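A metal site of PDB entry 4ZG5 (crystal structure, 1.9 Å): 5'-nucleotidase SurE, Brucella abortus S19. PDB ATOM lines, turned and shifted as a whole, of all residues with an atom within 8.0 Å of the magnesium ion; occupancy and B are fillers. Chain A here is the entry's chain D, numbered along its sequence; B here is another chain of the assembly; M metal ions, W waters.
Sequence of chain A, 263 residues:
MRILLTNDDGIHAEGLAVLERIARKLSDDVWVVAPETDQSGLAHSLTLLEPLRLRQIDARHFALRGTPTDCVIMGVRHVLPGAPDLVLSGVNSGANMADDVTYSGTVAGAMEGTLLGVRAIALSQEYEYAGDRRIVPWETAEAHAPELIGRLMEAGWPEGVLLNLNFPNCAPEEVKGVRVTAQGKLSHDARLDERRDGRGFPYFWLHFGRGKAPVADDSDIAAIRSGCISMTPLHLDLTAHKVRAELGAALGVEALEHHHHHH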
ATOM      1  N   ASN A   7      -2.760  -5.718  -3.338  1.00  0.00           N
ATOM      2  CA  ASN A   7      -3.330  -5.501  -4.703  1.00  0.00           C
ATOM      3  C   ASN A   7      -3.019  -6.670  -5.593  1.00  0.00           C
ATOM      4  O   ASN A   7      -2.491  -7.697  -5.103  1.00  0.00           O
ATOM      5  CB  ASN A   7      -2.874  -4.163  -5.367  1.00  0.00           C
ATOM      6  CG  ASN A   7      -1.430  -4.199  -5.851  1.00  0.00           C
ATOM      7  OD1 ASN A   7      -0.664  -5.135  -5.612  1.00  0.00           O
ATOM      8  ND2 ASN A   7      -1.047  -3.160  -6.584  1.00  0.00           N
ATOM      9  N   ASP A   8      -3.408  -6.575  -6.875  1.00  0.00           N
ATOM     10  CA  ASP A   8      -3.022  -7.564  -7.879  1.00  0.00           C
ATOM     11  C   ASP A   8      -2.098  -7.015  -8.958  1.00  0.00           C
ATOM     12  O   ASP A   8      -1.530  -7.767  -9.755  1.00  0.00           O
ATOM     13  CB  ASP A   8      -4.284  -8.236  -8.431  1.00  0.00           C
ATOM     14  CG  ASP A   8      -4.721  -7.694  -9.752  1.00  0.00           C
ATOM     15  OD1 ASP A   8      -5.204  -8.571 -10.499  1.00  0.00           O
ATOM     16  OD2 ASP A   8      -4.588  -6.510 -10.092  1.00  0.00           O
ATOM     17  N   ASP A   9      -1.878  -5.678  -8.938  1.00  0.00           N
ATOM     18  CA  ASP A   9      -1.027  -5.052  -9.891  1.00  0.00           C
ATOM     19  C   ASP A   9       0.419  -5.123  -9.523  1.00  0.00           C
ATOM     20  O   ASP A   9       1.249  -4.826 -10.350  1.00  0.00           O
ATOM     21  CB  ASP A   9      -1.440  -3.596 -10.148  1.00  0.00           C
ATOM     22  CG  ASP A   9      -2.832  -3.470 -10.773  1.00  0.00           C
ATOM     23  OD1 ASP A   9      -3.370  -4.408 -11.414  1.00  0.00           O
ATOM     24  OD2 ASP A   9      -3.403  -2.370 -10.544  1.00  0.00           O
ATOM     25  N   GLY A  10       0.762  -5.412  -8.276  1.00  0.00           N
ATOM     26  CA  GLY A  10       2.135  -5.467  -7.843  1.00  0.00           C
ATOM     27  C   GLY A  10       2.584  -4.349  -6.916  1.00  0.00           C
ATOM     28  O   GLY A  10       2.005  -3.270  -6.948  1.00  0.00           O
ATOM     29  N   ALA A  13       3.118  -0.890  -8.396  1.00  0.00           N
ATOM     30  CA  ALA A  13       2.059  -0.263  -9.271  1.00  0.00           C
ATOM     31  C   ALA A  13       1.515   1.037  -8.698  1.00  0.00           C
ATOM     32  O   ALA A  13       1.353   1.197  -7.465  1.00  0.00           O
ATOM     33  CB  ALA A  13       0.912  -1.266  -9.438  1.00  0.00           C
ATOM     34  N   ASP A  38       2.536  -8.341 -11.622  1.00  0.00           N
ATOM     35  CA  ASP A  38       1.123  -8.524 -12.071  1.00  0.00           C
ATOM     36  C   ASP A  38       0.454  -9.874 -11.934  1.00  0.00           C
ATOM     37  O   ASP A  38       1.013 -10.950 -12.193  1.00  0.00           O
ATOM     38  CB  ASP A  38       0.941  -8.055 -13.464  1.00  0.00           C
ATOM     39  CG  ASP A  38      -0.544  -7.708 -13.732  1.00  0.00           C
ATOM     40  OD1 ASP A  38      -1.013  -6.580 -13.234  1.00  0.00           O
ATOM     41  OD2 ASP A  38      -1.211  -8.646 -14.303  1.00  0.00           O
ATOM     42  N   GLN A  39      -0.775  -9.852 -11.464  1.00  0.00           N
ATOM     43  CA  GLN A  39      -1.413 -11.094 -11.083  1.00  0.00           C
ATOM     44  C   GLN A  39      -2.728 -11.272 -11.865  1.00  0.00           C
ATOM     45  O   GLN A  39      -3.664 -11.927 -11.280  1.00  0.00           O
ATOM     46  CB  GLN A  39      -1.719 -11.123  -9.531  1.00  0.00           C
ATOM     47  CG  GLN A  39      -0.471 -11.013  -8.645  1.00  0.00           C
ATOM     48  CD  GLN A  39       0.363 -12.312  -8.635  1.00  0.00           C
ATOM     49  OE1 GLN A  39       1.561 -12.302  -8.846  1.00  0.00           O
ATOM     50  NE2 GLN A  39      -0.277 -13.404  -8.413  1.00  0.00           N
ATOM     51  N   SER A  40      -2.846 -10.761 -13.132  1.00  0.00           N
ATOM     52  CA  SER A  40      -4.193 -10.770 -13.715  1.00  0.00           C
ATOM     53  C   SER A  40      -4.747 -12.207 -13.760  1.00  0.00           C
ATOM     54  O   SER A  40      -4.018 -13.086 -14.095  1.00  0.00           O
ATOM     55  CB  SER A  40      -4.174 -10.299 -15.163  1.00  0.00           C
ATOM     56  OG  SER A  40      -3.692  -8.975 -15.234  1.00  0.00           O
ATOM     57  N   GLY A  41      -6.046 -12.389 -13.488  1.00  0.00           N
ATOM     58  CA  GLY A  41      -6.686 -13.666 -13.639  1.00  0.00           C
ATOM     59  C   GLY A  41      -6.433 -14.712 -12.557  1.00  0.00           C
ATOM     60  O   GLY A  41      -6.774 -15.838 -12.734  1.00  0.00           O
ATOM     61  N   GLY A  90      -6.365  -3.110  -3.733  1.00  0.00           N
ATOM     62  CA  GLY A  90      -6.395  -2.223  -4.880  1.00  0.00           C
ATOM     63  C   GLY A  90      -5.374  -1.083  -4.762  1.00  0.00           C
ATOM     64  O   GLY A  90      -4.257  -1.311  -4.269  1.00  0.00           O
ATOM     65  N   VAL A  91      -5.651   0.089  -5.343  1.00  0.00           N
ATOM     66  CA  VAL A  91      -6.731   0.382  -6.253  1.00  0.00           C
ATOM     67  C   VAL A  91      -6.386  -0.225  -7.597  1.00  0.00           C
ATOM     68  O   VAL A  91      -5.345   0.146  -8.218  1.00  0.00           O
ATOM     69  CB  VAL A  91      -6.988   1.940  -6.438  1.00  0.00           C
ATOM     70  CG1 VAL A  91      -8.217   2.155  -7.290  1.00  0.00           C
ATOM     71  CG2 VAL A  91      -7.148   2.623  -5.079  1.00  0.00           C
ATOM     72  N   ASN A  92      -7.189  -1.173  -8.048  1.00  0.00           N
ATOM     73  CA  ASN A  92      -6.863  -1.788  -9.303  1.00  0.00           C
ATOM     74  C   ASN A  92      -6.921  -0.861 -10.492  1.00  0.00           C
ATOM     75  O   ASN A  92      -7.812  -0.011 -10.590  1.00  0.00           O
ATOM     76  CB  ASN A  92      -7.782  -2.990  -9.624  1.00  0.00           C
ATOM     77  CG  ASN A  92      -7.236  -3.840 -10.755  1.00  0.00           C
ATOM     78  OD1 ASN A  92      -6.068  -4.408 -10.744  1.00  0.00           O
ATOM     79  ND2 ASN A  92      -8.074  -3.967 -11.792  1.00  0.00           N
ATOM     80  N   SER A  93      -5.996  -1.112 -11.428  1.00  0.00           N
ATOM     81  CA  SER A  93      -6.025  -0.477 -12.767  1.00  0.00           C
ATOM     82  C   SER A  93      -7.063  -1.209 -13.625  1.00  0.00           C
ATOM     83  O   SER A  93      -6.748  -2.233 -14.203  1.00  0.00           O
ATOM     84  CB  SER A  93      -4.649  -0.542 -13.417  1.00  0.00           C
ATOM     85  OG  SER A  93      -4.727   0.083 -14.690  1.00  0.00           O
ATOM     86  N   GLY A  94      -8.292  -0.709 -13.611  1.00  0.00           N
ATOM     87  CA  GLY A  94      -9.388  -1.324 -14.392  1.00  0.00           C
ATOM     88  C   GLY A  94     -10.461  -1.750 -13.383  1.00  0.00           C
ATOM     89  O   GLY A  94     -10.191  -2.111 -12.243  1.00  0.00           O
ATOM     90  N   ALA A  95     -11.681  -1.713 -13.845  1.00  0.00           N
ATOM     91  CA  ALA A  95     -12.806  -2.088 -13.081  1.00  0.00           C
ATOM     92  C   ALA A  95     -12.880  -3.625 -12.831  1.00  0.00           C
ATOM     93  O   ALA A  95     -12.284  -4.407 -13.556  1.00  0.00           O
ATOM     94  CB  ALA A  95     -14.058  -1.643 -13.802  1.00  0.00           C
ATOM     95  N   ASN A  96     -13.507  -3.982 -11.738  1.00  0.00           N
ATOM     96  CA  ASN A  96     -13.802  -5.393 -11.403  1.00  0.00           C
ATOM     97  C   ASN A  96     -15.288  -5.527 -11.084  1.00  0.00           C
ATOM     98  O   ASN A  96     -15.740  -5.257 -10.022  1.00  0.00           O
ATOM     99  CB  ASN A  96     -12.947  -5.833 -10.190  1.00  0.00           C
ATOM    100  CG  ASN A  96     -11.524  -6.156 -10.548  1.00  0.00           C
ATOM    101  OD1 ASN A  96     -10.586  -5.403 -10.239  1.00  0.00           O
ATOM    102  ND2 ASN A  96     -11.378  -7.163 -11.299  1.00  0.00           N
ATOM    103  N   SER A 104     -11.118 -12.155 -10.236  1.00  0.00           N
ATOM    104  CA  SER A 104     -10.331 -11.005  -9.854  1.00  0.00           C
ATOM    105  C   SER A 104      -9.418 -11.253  -8.615  1.00  0.00           C
ATOM    106  O   SER A 104      -9.928 -11.640  -7.534  1.00  0.00           O
ATOM    107  CB  SER A 104     -11.264  -9.858  -9.472  1.00  0.00           C
ATOM    108  OG  SER A 104     -10.563  -8.775  -8.857  1.00  0.00           O
ATOM    109  N   GLY A 105      -8.126 -11.032  -8.807  1.00  0.00           N
ATOM    110  CA  GLY A 105      -7.198 -11.095  -7.695  1.00  0.00           C
ATOM    111  C   GLY A 105      -7.450  -9.954  -6.720  1.00  0.00           C
ATOM    112  O   GLY A 105      -7.300 -10.111  -5.487  1.00  0.00           O
ATOM    113  N   THR A 106      -7.823  -8.779  -7.248  1.00  0.00           N
ATOM    114  CA  THR A 106      -8.133  -7.683  -6.348  1.00  0.00           C
ATOM    115  C   THR A 106      -9.289  -8.045  -5.395  1.00  0.00           C
ATOM    116  O   THR A 106      -9.214  -7.852  -4.174  1.00  0.00           O
ATOM    117  CB  THR A 106      -8.471  -6.407  -7.133  1.00  0.00           C
ATOM    118  OG1 THR A 106      -7.405  -6.137  -8.033  1.00  0.00           O
ATOM    119  CG2 THR A 106      -8.697  -5.251  -6.185  1.00  0.00           C
ATOM    120  N   SER A 124     -11.419  -0.559  -7.205  1.00  0.00           N
ATOM    121  CA  SER A 124     -10.966  -0.635  -8.576  1.00  0.00           C
ATOM    122  C   SER A 124     -11.315   0.663  -9.282  1.00  0.00           C
ATOM    123  O   SER A 124     -12.402   1.244  -9.066  1.00  0.00           O
ATOM    124  CB  SER A 124     -11.601  -1.814  -9.307  1.00  0.00           C
ATOM    125  OG  SER A 124     -11.338  -3.108  -8.689  1.00  0.00           O
ATOM    126  N   ARG A 134      -3.060   3.257 -20.973  1.00  0.00           N
ATOM    127  CA  ARG A 134      -4.118   3.511 -20.036  1.00  0.00           C
ATOM    128  C   ARG A 134      -3.976   4.903 -19.460  1.00  0.00           C
ATOM    129  O   ARG A 134      -2.914   5.290 -19.026  1.00  0.00           O
ATOM    130  CB  ARG A 134      -4.067   2.555 -18.859  1.00  0.00           C
ATOM    131  CG  ARG A 134      -4.066   1.098 -19.204  1.00  0.00           C
ATOM    132  CD  ARG A 134      -4.296   0.255 -18.026  1.00  0.00           C
ATOM    133  NE  ARG A 134      -4.290  -1.114 -18.561  1.00  0.00           N
ATOM    134  CZ  ARG A 134      -4.619  -2.196 -17.884  1.00  0.00           C
ATOM    135  NH1 ARG A 134      -4.888  -2.114 -16.579  1.00  0.00           N
ATOM    136  NH2 ARG A 134      -4.627  -3.364 -18.498  1.00  0.00           N
ATOM    137  N   TRP A 138      -6.770   8.214 -11.394  1.00  0.00           N
ATOM    138  CA  TRP A 138      -6.538   7.815 -10.016  1.00  0.00           C
ATOM    139  C   TRP A 138      -7.050   8.795  -9.022  1.00  0.00           C
ATOM    140  O   TRP A 138      -7.473   8.427  -7.924  1.00  0.00           O
ATOM    141  CB  TRP A 138      -5.024   7.607  -9.785  1.00  0.00           C
ATOM    142  CG  TRP A 138      -4.364   6.509 -10.518  1.00  0.00           C
ATOM    143  CD1 TRP A 138      -3.360   6.632 -11.505  1.00  0.00           C
ATOM    144  CD2 TRP A 138      -4.631   5.057 -10.442  1.00  0.00           C
ATOM    145  NE1 TRP A 138      -3.004   5.397 -11.962  1.00  0.00           N
ATOM    146  CE2 TRP A 138      -3.738   4.420 -11.314  1.00  0.00           C
ATOM    147  CE3 TRP A 138      -5.546   4.279  -9.726  1.00  0.00           C
ATOM    148  CZ2 TRP A 138      -3.728   3.007 -11.488  1.00  0.00           C
ATOM    149  CZ3 TRP A 138      -5.515   2.922  -9.848  1.00  0.00           C
ATOM    150  CH2 TRP A 138      -4.612   2.282 -10.729  1.00  0.00           C
ATOM    151  N   ARG B 199      -4.074 -10.107 -25.152  1.00  0.00           N
ATOM    152  CA  ARG B 199      -4.372  -8.754 -24.649  1.00  0.00           C
ATOM    153  C   ARG B 199      -3.638  -7.622 -25.315  1.00  0.00           C
ATOM    154  O   ARG B 199      -3.625  -6.504 -24.802  1.00  0.00           O
ATOM    155  CB  ARG B 199      -4.152  -8.762 -23.139  1.00  0.00           C
ATOM    156  CG  ARG B 199      -5.005  -9.842 -22.511  1.00  0.00           C
ATOM    157  CD  ARG B 199      -4.982  -9.851 -20.995  1.00  0.00           C
ATOM    158  NE  ARG B 199      -3.629 -10.088 -20.505  1.00  0.00           N
ATOM    159  CZ  ARG B 199      -3.198  -9.758 -19.286  1.00  0.00           C
ATOM    160  NH1 ARG B 199      -3.998  -9.124 -18.417  1.00  0.00           N
ATOM    161  NH2 ARG B 199      -1.972 -10.051 -18.946  1.00  0.00           N
HETATM  162 MG    MG M   1      -4.818  -5.504 -11.764  1.00  0.00          MG
HETATM  163  O   HOH W   1      -5.126  -4.433 -13.551  1.00  0.00           O
HETATM  164  O   HOH W   2      -3.753  -6.869 -12.891  1.00  0.00           O
HETATM  165  O   HOH W   3      -6.387  -6.737 -12.365  1.00  0.00           O
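OD2 of Asp 9 sits at hydrogen-bond distance from N of Ser 93.
The side-chain hydroxyl (OG1) of Thr 106 lies close to the side-chain amide oxygen (OD1) of Asn 92, at 3.5 Å.
OD1 of Asn 96 is in hydrogen-bond range of ND2 of Asn 92 (3.3 Å).
The backbone carbonyl oxygen (O) of Gly 94 lies within hydrogen-bond range of the side-chain amide nitrogen (ND2) of Asn 92, at 2.9 Å.
The backbone carbonyl oxygen (O) of Asp 8 sits at hydrogen-bond distance from the backbone NH (N) of Gln 39.
Three residues have an atom within 4 Å of the magnesium ion: Asp 8, Asp 9 and Asn 92.
The magnesium ion is bound by OD1 of Asp 9 (1.8 Å), OD1 of Asn 92 (2.0 Å), OD2 of Asp 8 (2.0 Å), water W2 (2.1 Å), water W3 (2.1 Å) and water W1 (2.1 Å).
Water W3 bridges the side-chain carboxylate (OD1) of Asp 8 and the side-chain amide nitrogen (ND2) of Asn 92.
Water W1 bridges O of Ser 93 (2.8 Å) and ND2 of Asn 92 (3.5 Å).
Water W2 lies within hydrogen-bond range of the side-chain carboxylate (OD1) of Asp 38 (2.8 Å), the side-chain hydroxyl (OG) of Ser 40 (3.2 Å) and the side-chain carboxylate (OD1) of Asp 8 (3.3 Å).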
